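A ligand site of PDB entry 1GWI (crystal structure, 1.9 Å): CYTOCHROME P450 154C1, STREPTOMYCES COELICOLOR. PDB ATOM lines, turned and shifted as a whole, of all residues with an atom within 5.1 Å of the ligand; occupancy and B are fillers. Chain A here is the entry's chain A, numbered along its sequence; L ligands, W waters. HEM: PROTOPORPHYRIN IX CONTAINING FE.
SD of Met 92 sits close to O1D of the ligand (3.8 Å). CD2 of Leu 56 touches O2A of the ligand, 3.8 Å away. Leu 93 touches the ligand. Leu 111 touches the ligand. Leu 238 touches the ligand (CD2 to CMD, 3.7 Å). Met 239 touches the ligand (CE to CBC, 3.7 Å). Ala 242 touches the ligand (O to NC, 3.7 Å). Gly 243 touches the ligand. Thr 246 touches the ligand. Thr 247 touches the ligand. Leu 250 touches the ligand (CD2 to CBB, 3.5 Å). Leu 283 touches the ligand (CD2 to CBB, 3.6 Å). Thr 287 touches the ligand (OG1 to CMB, 3.9 Å). Pro 288 touches the ligand (CD to CMB, 3.9 Å). Val 292 touches the ligand (CG1 to O2A, 3.4 Å). Ser 347 touches the ligand (O to CMA, 3.2 Å). CE2 of Phe 348 touches CBB of the ligand, at 3.5 Å. Gly 349 touches the ligand. Pro 356 touches the ligand. Gly 357 touches the ligand (CA to CBC, 3.6 Å). Ser 361 touches the ligand (OG to CBB, 3.5 Å). Hydrophobic or aromatic side chains within 4 Å of the ligand: Leu 56, Met 92, Leu 93, His 100, Leu 111, Leu 238, Met 239, Ala 242, Leu 250, Leu 283, Pro 288, Val 292, Tyr 318, Phe 348, His 353 and Pro 356.
Water W3 bridges O1A of the ligand (2.7 Å) and NZ of Lys 63 (2.9 Å).
The guanidinium group (NH1) of Arg 104 lies within salt-bridge range of an oxygen (O1D) of the ligand, at 2.8 Å. A ring nitrogen (ND1) of His 353 sits at hydrogen-bond distance from an oxygen (O2D) of the ligand. The guanidinium group of Arg 295 is in salt-bridge range of an oxygen (O1A) of the ligand. The side-chain sulfur of Cys 355 is bound to an iron atom (FE) of the ligand (2.5 Å). A ring nitrogen (NE2) of His 100 is in hydrogen-bond range of an oxygen (O1D) of the ligand (2.7 Å). The side-chain hydroxyl of Tyr 318 is in hydrogen-bond range of an oxygen (O2A) of the ligand, at 2.7 Å.
O of Gly 243 sits at hydrogen-bond distance from OG1 of Thr 247, 2.6 Å away. The backbone carbonyl oxygen (O) of Val 316 sits at hydrogen-bond distance from the backbone NH (N) of Val 292 (3.0 Å). NH2 of Arg 104 lies within hydrogen-bond range of O of Val 354, 2.8 Å away. A ring nitrogen (ND1) of His 353 is in hydrogen-bond range of a ring nitrogen (NE2) of His 100 (3.1 Å). The side-chain hydroxyl of Thr 246 lies close to the backbone carbonyl oxygen of Gly 243 (3.4 Å). The backbone carbonyl oxygen (O) of Met 92 lies close to a ring nitrogen (NE2) of His 100 (3.4 Å). O of Gly 357 is in hydrogen-bond range of OG of Ser 361 (3.1 Å). The backbone NH of Thr 289 lies close to the side-chain hydroxyl of Thr 287, at 3.1 Å.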
ATOM      1  N   LEU A  56      27.326  -2.383  -9.240  1.00  0.00           N
ATOM      2  CA  LEU A  56      26.999  -2.584 -10.642  1.00  0.00           C
ATOM      3  C   LEU A  56      28.253  -2.730 -11.501  1.00  0.00           C
ATOM      4  O   LEU A  56      28.195  -3.298 -12.598  1.00  0.00           O
ATOM      5  CB  LEU A  56      26.134  -1.432 -11.161  1.00  0.00           C
ATOM      6  CG  LEU A  56      24.649  -1.520 -10.789  1.00  0.00           C
ATOM      7  CD1 LEU A  56      23.940  -0.231 -11.183  1.00  0.00           C
ATOM      8  CD2 LEU A  56      24.019  -2.716 -11.496  1.00  0.00           C
ATOM      9  N   LYS A  63      25.778 -12.526 -12.740  1.00  0.00           N
ATOM     10  CA  LYS A  63      24.420 -12.972 -13.038  1.00  0.00           C
ATOM     11  C   LYS A  63      24.310 -14.500 -12.905  1.00  0.00           C
ATOM     12  O   LYS A  63      23.230 -15.021 -12.621  1.00  0.00           O
ATOM     13  CB  LYS A  63      24.012 -12.557 -14.451  1.00  0.00           C
ATOM     14  CG  LYS A  63      23.926 -11.039 -14.691  1.00  0.00           C
ATOM     15  CD  LYS A  63      22.947 -10.371 -13.742  1.00  0.00           C
ATOM     16  CE  LYS A  63      22.571  -8.972 -14.224  1.00  0.00           C
ATOM     17  NZ  LYS A  63      21.747  -9.026 -15.469  1.00  0.00           N
ATOM     18  N   MET A  92      21.895 -11.534 -23.190  1.00  0.00           N
ATOM     19  CA  MET A  92      22.942 -10.662 -22.630  1.00  0.00           C
ATOM     20  C   MET A  92      22.666 -10.439 -21.150  1.00  0.00           C
ATOM     21  O   MET A  92      23.536 -10.037 -20.384  1.00  0.00           O
ATOM     22  CB  MET A  92      22.956  -9.312 -23.377  1.00  0.00           C
ATOM     23  CG  MET A  92      21.658  -8.524 -23.255  1.00  0.00           C
ATOM     24  SD  MET A  92      21.658  -6.975 -24.185  1.00  0.00           S
ATOM     25  CE  MET A  92      21.342  -7.568 -25.852  1.00  0.00           C
ATOM     26  N   LEU A  93      21.431 -10.718 -20.755  1.00  0.00           N
ATOM     27  CA  LEU A  93      20.988 -10.561 -19.384  1.00  0.00           C
ATOM     28  C   LEU A  93      21.595 -11.551 -18.385  1.00  0.00           C
ATOM     29  O   LEU A  93      21.871 -11.191 -17.240  1.00  0.00           O
ATOM     30  CB  LEU A  93      19.466 -10.656 -19.346  1.00  0.00           C
ATOM     31  CG  LEU A  93      18.716 -10.348 -18.057  1.00  0.00           C
ATOM     32  CD1 LEU A  93      18.860  -8.869 -17.737  1.00  0.00           C
ATOM     33  CD2 LEU A  93      17.253 -10.723 -18.221  1.00  0.00           C
ATOM     34  N   HIS A 100      29.555 -11.433 -22.240  1.00  0.00           N
ATOM     35  CA  HIS A 100      28.621 -10.311 -22.260  1.00  0.00           C
ATOM     36  C   HIS A 100      29.084  -9.233 -23.228  1.00  0.00           C
ATOM     37  O   HIS A 100      28.281  -8.707 -24.000  1.00  0.00           O
ATOM     38  CB  HIS A 100      28.476  -9.738 -20.851  1.00  0.00           C
ATOM     39  CG  HIS A 100      27.468  -8.629 -20.754  1.00  0.00           C
ATOM     40  ND1 HIS A 100      27.821  -7.301 -20.654  1.00  0.00           N
ATOM     41  CD2 HIS A 100      26.118  -8.656 -20.757  1.00  0.00           C
ATOM     42  CE1 HIS A 100      26.735  -6.551 -20.597  1.00  0.00           C
ATOM     43  NE2 HIS A 100      25.679  -7.354 -20.651  1.00  0.00           N
ATOM     44  N   ARG A 104      26.903  -7.520 -26.308  1.00  0.00           N
ATOM     45  CA  ARG A 104      26.659  -6.084 -26.330  1.00  0.00           C
ATOM     46  C   ARG A 104      27.273  -5.383 -27.544  1.00  0.00           C
ATOM     47  O   ARG A 104      26.623  -4.538 -28.154  1.00  0.00           O
ATOM     48  CB  ARG A 104      27.148  -5.432 -25.022  1.00  0.00           C
ATOM     49  CG  ARG A 104      26.313  -5.816 -23.796  1.00  0.00           C
ATOM     50  CD  ARG A 104      24.818  -5.475 -23.992  1.00  0.00           C
ATOM     51  NE  ARG A 104      24.590  -4.046 -24.156  1.00  0.00           N
ATOM     52  CZ  ARG A 104      24.161  -3.227 -23.201  1.00  0.00           C
ATOM     53  NH1 ARG A 104      23.896  -3.686 -21.978  1.00  0.00           N
ATOM     54  NH2 ARG A 104      24.006  -1.935 -23.454  1.00  0.00           N
ATOM     55  N   LEU A 111      21.257  -2.019 -32.846  1.00  0.00           N
ATOM     56  CA  LEU A 111      20.445  -1.051 -32.097  1.00  0.00           C
ATOM     57  C   LEU A 111      21.382   0.116 -31.811  1.00  0.00           C
ATOM     58  O   LEU A 111      21.981   0.219 -30.729  1.00  0.00           O
ATOM     59  CB  LEU A 111      19.938  -1.657 -30.790  1.00  0.00           C
ATOM     60  CG  LEU A 111      19.053  -0.729 -29.953  1.00  0.00           C
ATOM     61  CD1 LEU A 111      17.852  -0.280 -30.778  1.00  0.00           C
ATOM     62  CD2 LEU A 111      18.597  -1.445 -28.691  1.00  0.00           C
ATOM     63  N   LEU A 238      13.996 -10.461 -25.577  1.00  0.00           N
ATOM     64  CA  LEU A 238      14.390  -9.675 -24.422  1.00  0.00           C
ATOM     65  C   LEU A 238      13.981  -8.220 -24.563  1.00  0.00           C
ATOM     66  O   LEU A 238      13.591  -7.579 -23.579  1.00  0.00           O
ATOM     67  CB  LEU A 238      15.903  -9.756 -24.206  1.00  0.00           C
ATOM     68  CG  LEU A 238      16.455  -9.044 -22.963  1.00  0.00           C
ATOM     69  CD1 LEU A 238      15.749  -9.549 -21.702  1.00  0.00           C
ATOM     70  CD2 LEU A 238      17.963  -9.296 -22.862  1.00  0.00           C
ATOM     71  N   MET A 239      14.064  -7.677 -25.776  1.00  0.00           N
ATOM     72  CA  MET A 239      13.689  -6.288 -26.018  1.00  0.00           C
ATOM     73  C   MET A 239      12.206  -6.075 -25.731  1.00  0.00           C
ATOM     74  O   MET A 239      11.806  -5.006 -25.287  1.00  0.00           O
ATOM     75  CB  MET A 239      14.022  -5.883 -27.446  1.00  0.00           C
ATOM     76  CG  MET A 239      15.514  -5.947 -27.748  1.00  0.00           C
ATOM     77  SD  MET A 239      15.924  -5.356 -29.384  1.00  0.00           S
ATOM     78  CE  MET A 239      17.207  -4.256 -28.997  1.00  0.00           C
ATOM     79  N   ALA A 242      11.890  -6.471 -21.801  1.00  0.00           N
ATOM     80  CA  ALA A 242      12.488  -5.369 -21.049  1.00  0.00           C
ATOM     81  C   ALA A 242      12.079  -3.965 -21.469  1.00  0.00           C
ATOM     82  O   ALA A 242      12.176  -3.030 -20.666  1.00  0.00           O
ATOM     83  CB  ALA A 242      14.012  -5.479 -21.118  1.00  0.00           C
ATOM     84  N   GLY A 243      11.605  -3.806 -22.691  1.00  0.00           N
ATOM     85  CA  GLY A 243      11.226  -2.473 -23.113  1.00  0.00           C
ATOM     86  C   GLY A 243       9.782  -2.087 -23.348  1.00  0.00           C
ATOM     87  O   GLY A 243       9.509  -0.922 -23.625  1.00  0.00           O
ATOM     88  N   THR A 246       8.125  -0.969 -19.543  1.00  0.00           N
ATOM     89  CA  THR A 246       8.951   0.100 -18.997  1.00  0.00           C
ATOM     90  C   THR A 246       8.655   1.392 -19.743  1.00  0.00           C
ATOM     91  O   THR A 246       8.419   2.432 -19.132  1.00  0.00           O
ATOM     92  CB  THR A 246      10.459  -0.218 -19.146  1.00  0.00           C
ATOM     93  OG1 THR A 246      10.721  -0.682 -20.474  1.00  0.00           O
ATOM     94  CG2 THR A 246      10.895  -1.273 -18.135  1.00  0.00           C
ATOM     95  N   THR A 247       8.665   1.331 -21.070  1.00  0.00           N
ATOM     96  CA  THR A 247       8.402   2.512 -21.877  1.00  0.00           C
ATOM     97  C   THR A 247       6.998   3.052 -21.587  1.00  0.00           C
ATOM     98  O   THR A 247       6.809   4.256 -21.462  1.00  0.00           O
ATOM     99  CB  THR A 247       8.549   2.191 -23.380  1.00  0.00           C
ATOM    100  OG1 THR A 247       9.861   1.662 -23.617  1.00  0.00           O
ATOM    101  CG2 THR A 247       8.387   3.459 -24.222  1.00  0.00           C
ATOM    102  N   LEU A 250       7.002   4.870 -18.396  1.00  0.00           N
ATOM    103  CA  LEU A 250       7.741   6.122 -18.454  1.00  0.00           C
ATOM    104  C   LEU A 250       6.763   7.213 -18.895  1.00  0.00           C
ATOM    105  O   LEU A 250       6.708   8.291 -18.311  1.00  0.00           O
ATOM    106  CB  LEU A 250       8.890   6.024 -19.456  1.00  0.00           C
ATOM    107  CG  LEU A 250       9.618   7.337 -19.774  1.00  0.00           C
ATOM    108  CD1 LEU A 250      10.239   7.913 -18.500  1.00  0.00           C
ATOM    109  CD2 LEU A 250      10.709   7.085 -20.828  1.00  0.00           C
ATOM    110  N   LEU A 283      12.314   9.625 -14.761  1.00  0.00           N
ATOM    111  CA  LEU A 283      13.124   8.413 -14.622  1.00  0.00           C
ATOM    112  C   LEU A 283      13.762   8.375 -13.233  1.00  0.00           C
ATOM    113  O   LEU A 283      13.852   7.314 -12.611  1.00  0.00           O
ATOM    114  CB  LEU A 283      14.225   8.395 -15.701  1.00  0.00           C
ATOM    115  CG  LEU A 283      13.759   8.031 -17.109  1.00  0.00           C
ATOM    116  CD1 LEU A 283      14.847   8.394 -18.143  1.00  0.00           C
ATOM    117  CD2 LEU A 283      13.445   6.538 -17.166  1.00  0.00           C
ATOM    118  N   THR A 287      10.995   5.880 -11.550  1.00  0.00           N
ATOM    119  CA  THR A 287      11.426   4.936 -12.568  1.00  0.00           C
ATOM    120  C   THR A 287      10.445   3.791 -12.712  1.00  0.00           C
ATOM    121  O   THR A 287       9.849   3.335 -11.735  1.00  0.00           O
ATOM    122  CB  THR A 287      12.806   4.334 -12.231  1.00  0.00           C
ATOM    123  OG1 THR A 287      13.127   3.346 -13.227  1.00  0.00           O
ATOM    124  CG2 THR A 287      12.787   3.670 -10.852  1.00  0.00           C
ATOM    125  N   PRO A 288      10.262   3.308 -13.945  1.00  0.00           N
ATOM    126  CA  PRO A 288       9.346   2.191 -14.235  1.00  0.00           C
ATOM    127  C   PRO A 288       9.909   0.887 -13.670  1.00  0.00           C
ATOM    128  O   PRO A 288       9.175  -0.087 -13.486  1.00  0.00           O
ATOM    129  CB  PRO A 288       9.303   2.159 -15.753  1.00  0.00           C
ATOM    130  CG  PRO A 288       9.594   3.573 -16.154  1.00  0.00           C
ATOM    131  CD  PRO A 288      10.698   3.946 -15.203  1.00  0.00           C
ATOM    132  N   THR A 289      11.211   0.868 -13.409  1.00  0.00           N
ATOM    133  CA  THR A 289      11.865  -0.321 -12.879  1.00  0.00           C
ATOM    134  C   THR A 289      12.331  -0.106 -11.442  1.00  0.00           C
ATOM    135  O   THR A 289      13.420   0.412 -11.194  1.00  0.00           O
ATOM    136  CB  THR A 289      13.061  -0.678 -13.778  1.00  0.00           C
ATOM    137  OG1 THR A 289      12.602  -0.790 -15.131  1.00  0.00           O
ATOM    138  CG2 THR A 289      13.689  -1.990 -13.352  1.00  0.00           C
ATOM    139  N   VAL A 292      15.663  -4.726  -9.710  1.00  0.00           N
ATOM    140  CA  VAL A 292      16.165  -5.568 -10.763  1.00  0.00           C
ATOM    141  C   VAL A 292      16.838  -6.808 -10.199  1.00  0.00           C
ATOM    142  O   VAL A 292      17.789  -6.717  -9.415  1.00  0.00           O
ATOM    143  CB  VAL A 292      17.178  -4.850 -11.678  1.00  0.00           C
ATOM    144  CG1 VAL A 292      17.846  -5.868 -12.591  1.00  0.00           C
ATOM    145  CG2 VAL A 292      16.447  -3.803 -12.544  1.00  0.00           C
ATOM    146  N   ARG A 295      21.633 -10.490  -8.845  1.00  0.00           N
ATOM    147  CA  ARG A 295      23.067 -10.707  -8.900  1.00  0.00           C
ATOM    148  C   ARG A 295      23.515 -11.551  -7.703  1.00  0.00           C
ATOM    149  O   ARG A 295      22.826 -11.585  -6.682  1.00  0.00           O
ATOM    150  CB  ARG A 295      23.804  -9.364  -8.933  1.00  0.00           C
ATOM    151  CG  ARG A 295      23.590  -8.578 -10.230  1.00  0.00           C
ATOM    152  CD  ARG A 295      24.305  -7.231 -10.200  1.00  0.00           C
ATOM    153  NE  ARG A 295      24.433  -6.648 -11.529  1.00  0.00           N
ATOM    154  CZ  ARG A 295      23.446  -6.049 -12.198  1.00  0.00           C
ATOM    155  NH1 ARG A 295      22.235  -5.944 -11.665  1.00  0.00           N
ATOM    156  NH2 ARG A 295      23.689  -5.528 -13.398  1.00  0.00           N
ATOM    157  N   VAL A 316      19.032  -4.735  -7.233  1.00  0.00           N
ATOM    158  CA  VAL A 316      19.318  -3.303  -7.243  1.00  0.00           C
ATOM    159  C   VAL A 316      17.982  -2.576  -7.176  1.00  0.00           C
ATOM    160  O   VAL A 316      17.156  -2.696  -8.076  1.00  0.00           O
ATOM    161  CB  VAL A 316      20.095  -2.889  -8.513  1.00  0.00           C
ATOM    162  CG1 VAL A 316      20.389  -1.388  -8.478  1.00  0.00           C
ATOM    163  CG2 VAL A 316      21.391  -3.679  -8.592  1.00  0.00           C
ATOM    164  N   TYR A 318      16.505   0.396  -7.799  1.00  0.00           N
ATOM    165  CA  TYR A 318      16.537   1.687  -8.491  1.00  0.00           C
ATOM    166  C   TYR A 318      15.436   2.645  -8.029  1.00  0.00           C
ATOM    167  O   TYR A 318      15.659   3.852  -7.946  1.00  0.00           O
ATOM    168  CB  TYR A 318      16.414   1.463 -10.001  1.00  0.00           C
ATOM    169  CG  TYR A 318      17.580   0.724 -10.606  1.00  0.00           C
ATOM    170  CD1 TYR A 318      17.505  -0.644 -10.876  1.00  0.00           C
ATOM    171  CD2 TYR A 318      18.761   1.395 -10.929  1.00  0.00           C
ATOM    172  CE1 TYR A 318      18.580  -1.321 -11.461  1.00  0.00           C
ATOM    173  CE2 TYR A 318      19.836   0.733 -11.513  1.00  0.00           C
ATOM    174  CZ  TYR A 318      19.740  -0.629 -11.776  1.00  0.00           C
ATOM    175  OH  TYR A 318      20.805  -1.270 -12.352  1.00  0.00           O
ATOM    176  N   ILE A 346      20.617   6.889 -12.327  1.00  0.00           N
ATOM    177  CA  ILE A 346      21.162   5.641 -12.873  1.00  0.00           C
ATOM    178  C   ILE A 346      19.992   4.689 -13.080  1.00  0.00           C
ATOM    179  O   ILE A 346      20.130   3.472 -12.909  1.00  0.00           O
ATOM    180  CB  ILE A 346      22.200   4.967 -11.929  1.00  0.00           C
ATOM    181  CG1 ILE A 346      21.588   4.747 -10.545  1.00  0.00           C
ATOM    182  CG2 ILE A 346      23.455   5.805 -11.845  1.00  0.00           C
ATOM    183  CD1 ILE A 346      22.369   3.778  -9.681  1.00  0.00           C
ATOM    184  N   SER A 347      18.834   5.238 -13.453  1.00  0.00           N
ATOM    185  CA  SER A 347      17.644   4.436 -13.675  1.00  0.00           C
ATOM    186  C   SER A 347      17.733   3.507 -14.896  1.00  0.00           C
ATOM    187  O   SER A 347      16.891   2.618 -15.052  1.00  0.00           O
ATOM    188  CB  SER A 347      16.413   5.332 -13.759  1.00  0.00           C
ATOM    189  OG  SER A 347      16.174   5.926 -12.494  1.00  0.00           O
ATOM    190  N   PHE A 348      18.725   3.726 -15.748  1.00  0.00           N
ATOM    191  CA  PHE A 348      18.912   2.888 -16.926  1.00  0.00           C
ATOM    192  C   PHE A 348      20.053   1.930 -16.601  1.00  0.00           C
ATOM    193  O   PHE A 348      20.559   1.214 -17.471  1.00  0.00           O
ATOM    194  CB  PHE A 348      19.306   3.716 -18.157  1.00  0.00           C
ATOM    195  CG  PHE A 348      18.130   4.323 -18.882  1.00  0.00           C
ATOM    196  CD1 PHE A 348      18.054   5.691 -19.093  1.00  0.00           C
ATOM    197  CD2 PHE A 348      17.121   3.505 -19.381  1.00  0.00           C
ATOM    198  CE1 PHE A 348      16.977   6.255 -19.788  1.00  0.00           C
ATOM    199  CE2 PHE A 348      16.035   4.062 -20.084  1.00  0.00           C
ATOM    200  CZ  PHE A 348      15.968   5.437 -20.287  1.00  0.00           C
ATOM    201  N   GLY A 349      20.466   1.933 -15.338  1.00  0.00           N
ATOM    202  CA  GLY A 349      21.554   1.062 -14.905  1.00  0.00           C
ATOM    203  C   GLY A 349      22.915   1.723 -14.966  1.00  0.00           C
ATOM    204  O   GLY A 349      23.031   2.918 -15.241  1.00  0.00           O
ATOM    205  N   PRO A 352      28.552  -2.475 -17.365  1.00  0.00           N
ATOM    206  CA  PRO A 352      28.340  -3.278 -18.577  1.00  0.00           C
ATOM    207  C   PRO A 352      26.896  -3.536 -18.997  1.00  0.00           C
ATOM    208  O   PRO A 352      26.559  -3.449 -20.174  1.00  0.00           O
ATOM    209  CB  PRO A 352      29.083  -4.577 -18.253  1.00  0.00           C
ATOM    210  CG  PRO A 352      30.166  -4.141 -17.294  1.00  0.00           C
ATOM    211  CD  PRO A 352      29.399  -3.200 -16.395  1.00  0.00           C
ATOM    212  N   HIS A 353      26.039  -3.845 -18.016  1.00  0.00           N
ATOM    213  CA  HIS A 353      24.629  -4.124 -18.279  1.00  0.00           C
ATOM    214  C   HIS A 353      23.712  -2.901 -18.486  1.00  0.00           C
ATOM    215  O   HIS A 353      22.493  -3.055 -18.503  1.00  0.00           O
ATOM    216  CB  HIS A 353      24.069  -4.990 -17.156  1.00  0.00           C
ATOM    217  CG  HIS A 353      24.623  -6.376 -17.127  1.00  0.00           C
ATOM    218  ND1 HIS A 353      24.126  -7.391 -17.927  1.00  0.00           N
ATOM    219  CD2 HIS A 353      25.638  -6.920 -16.412  1.00  0.00           C
ATOM    220  CE1 HIS A 353      24.821  -8.494 -17.703  1.00  0.00           C
ATOM    221  NE2 HIS A 353      25.737  -8.233 -16.793  1.00  0.00           N
ATOM    222  N   VAL A 354      24.295  -1.717 -18.638  1.00  0.00           N
ATOM    223  CA  VAL A 354      23.478  -0.516 -18.834  1.00  0.00           C
ATOM    224  C   VAL A 354      22.470  -0.689 -19.977  1.00  0.00           C
ATOM    225  O   VAL A 354      22.823  -1.163 -21.062  1.00  0.00           O
ATOM    226  CB  VAL A 354      24.354   0.731 -19.086  1.00  0.00           C
ATOM    227  CG1 VAL A 354      25.095   0.589 -20.417  1.00  0.00           C
ATOM    228  CG2 VAL A 354      23.498   1.993 -19.068  1.00  0.00           C
ATOM    229  N   CYS A 355      21.229  -0.317 -19.731  1.00  0.00           N
ATOM    230  CA  CYS A 355      20.156  -0.427 -20.718  1.00  0.00           C
ATOM    231  C   CYS A 355      20.468   0.035 -22.145  1.00  0.00           C
ATOM    232  O   CYS A 355      20.743   1.207 -22.380  1.00  0.00           O
ATOM    233  CB  CYS A 355      18.924   0.338 -20.234  1.00  0.00           C
ATOM    234  SG  CYS A 355      17.567   0.285 -21.407  1.00  0.00           S
ATOM    235  N   PRO A 356      20.418  -0.884 -23.137  1.00  0.00           N
ATOM    236  CA  PRO A 356      20.689  -0.503 -24.519  1.00  0.00           C
ATOM    237  C   PRO A 356      19.470   0.157 -25.159  1.00  0.00           C
ATOM    238  O   PRO A 356      19.512   0.605 -26.313  1.00  0.00           O
ATOM    239  CB  PRO A 356      21.019  -1.838 -25.183  1.00  0.00           C
ATOM    240  CG  PRO A 356      20.113  -2.781 -24.452  1.00  0.00           C
ATOM    241  CD  PRO A 356      20.308  -2.348 -23.008  1.00  0.00           C
ATOM    242  N   GLY A 357      18.372   0.189 -24.419  1.00  0.00           N
ATOM    243  CA  GLY A 357      17.148   0.801 -24.934  1.00  0.00           C
ATOM    244  C   GLY A 357      16.943   2.206 -24.397  1.00  0.00           C
ATOM    245  O   GLY A 357      15.856   2.766 -24.533  1.00  0.00           O
ATOM    246  N   LEU A 360      16.124   4.603 -27.288  1.00  0.00           N
ATOM    247  CA  LEU A 360      14.814   4.288 -27.840  1.00  0.00           C
ATOM    248  C   LEU A 360      13.669   4.788 -26.947  1.00  0.00           C
ATOM    249  O   LEU A 360      12.744   5.449 -27.427  1.00  0.00           O
ATOM    250  CB  LEU A 360      14.667   2.768 -28.055  1.00  0.00           C
ATOM    251  CG  LEU A 360      13.320   2.335 -28.649  1.00  0.00           C
ATOM    252  CD1 LEU A 360      13.139   3.003 -30.000  1.00  0.00           C
ATOM    253  CD2 LEU A 360      13.270   0.812 -28.790  1.00  0.00           C
ATOM    254  N   SER A 361      13.741   4.469 -25.648  1.00  0.00           N
ATOM    255  CA  SER A 361      12.694   4.903 -24.719  1.00  0.00           C
ATOM    256  C   SER A 361      12.625   6.435 -24.618  1.00  0.00           C
ATOM    257  O   SER A 361      11.541   7.008 -24.576  1.00  0.00           O
ATOM    258  CB  SER A 361      12.943   4.304 -23.320  1.00  0.00           C
ATOM    259  OG  SER A 361      14.203   4.698 -22.802  1.00  0.00           O
HETATM  260  CHA HEM L   1      18.482  -3.432 -19.053  1.00  0.00           C
HETATM  261  CHB HEM L   1      15.876   0.254 -17.406  1.00  0.00           C
HETATM  262  CHC HEM L   1      13.654   0.540 -21.676  1.00  0.00           C
HETATM  263  CHD HEM L   1      16.218  -3.177 -23.284  1.00  0.00           C
HETATM  264  C1A HEM L   1      18.007  -2.445 -18.226  1.00  0.00           C
HETATM  265  C2A HEM L   1      18.476  -2.171 -16.871  1.00  0.00           C
HETATM  266  C3A HEM L   1      17.734  -1.148 -16.400  1.00  0.00           C
HETATM  267  C4A HEM L   1      16.812  -0.744 -17.458  1.00  0.00           C
HETATM  268  CMA HEM L   1      17.800  -0.465 -15.028  1.00  0.00           C
HETATM  269  CAA HEM L   1      19.624  -2.974 -16.199  1.00  0.00           C
HETATM  270  CBA HEM L   1      19.326  -3.671 -14.881  1.00  0.00           C
HETATM  271  CGA HEM L   1      20.610  -4.059 -14.135  1.00  0.00           C
HETATM  272  O1A HEM L   1      21.570  -4.503 -14.869  1.00  0.00           O
HETATM  273  O2A HEM L   1      20.654  -3.908 -12.915  1.00  0.00           O
HETATM  274  C1B HEM L   1      15.022   0.641 -18.405  1.00  0.00           C
HETATM  275  C2B HEM L   1      14.043   1.722 -18.294  1.00  0.00           C
HETATM  276  C3B HEM L   1      13.408   1.808 -19.497  1.00  0.00           C
HETATM  277  C4B HEM L   1      13.994   0.787 -20.356  1.00  0.00           C
HETATM  278  CMB HEM L   1      13.823   2.563 -17.025  1.00  0.00           C
HETATM  279  CAB HEM L   1      12.281   2.764 -19.957  1.00  0.00           C
HETATM  280  CBB HEM L   1      12.570   4.258 -19.766  1.00  0.00           C
HETATM  281  C1C HEM L   1      14.178  -0.440 -22.494  1.00  0.00           C
HETATM  282  C2C HEM L   1      13.771  -0.649 -23.893  1.00  0.00           C
HETATM  283  C3C HEM L   1      14.482  -1.687 -24.352  1.00  0.00           C
HETATM  284  C4C HEM L   1      15.333  -2.128 -23.249  1.00  0.00           C
HETATM  285  CMC HEM L   1      12.706   0.221 -24.637  1.00  0.00           C
HETATM  286  CAC HEM L   1      14.457  -2.340 -25.749  1.00  0.00           C
HETATM  287  CBC HEM L   1      15.611  -1.932 -26.672  1.00  0.00           C
HETATM  288  C1D HEM L   1      17.042  -3.614 -22.281  1.00  0.00           C
HETATM  289  C2D HEM L   1      17.960  -4.732 -22.360  1.00  0.00           C
HETATM  290  C3D HEM L   1      18.606  -4.809 -21.178  1.00  0.00           C
HETATM  291  C4D HEM L   1      18.081  -3.723 -20.348  1.00  0.00           C
HETATM  292  CMD HEM L   1      18.139  -5.638 -23.598  1.00  0.00           C
HETATM  293  CAD HEM L   1      19.684  -5.835 -20.765  1.00  0.00           C
HETATM  294  CBD HEM L   1      21.101  -5.194 -20.698  1.00  0.00           C
HETATM  295  CGD HEM L   1      22.159  -6.177 -20.284  1.00  0.00           C
HETATM  296  O1D HEM L   1      23.252  -6.187 -20.881  1.00  0.00           O
HETATM  297  O2D HEM L   1      21.845  -6.922 -19.330  1.00  0.00           O
HETATM  298  NA  HEM L   1      17.026  -1.565 -18.556  1.00  0.00           N
HETATM  299  NB  HEM L   1      14.951   0.089 -19.679  1.00  0.00           N
HETATM  300  NC  HEM L   1      15.138  -1.336 -22.137  1.00  0.00           N
HETATM  301  ND  HEM L   1      17.113  -3.005 -21.018  1.00  0.00           N
HETATM  302 FE   HEM L   1      16.062  -1.454 -20.351  1.00  0.00          FE
HETATM  303  O   HOH W   1      23.297  -1.886 -15.254  1.00  0.00           O
HETATM  304  O   HOH W   2      10.535  -0.986 -26.685  1.00  0.00           O
HETATM  305  O   HOH W   3      20.952  -6.444 -16.644  1.00  0.00           O
HETATM  306  O   HOH W   4      14.479  -2.999 -19.367  1.00  0.00           O
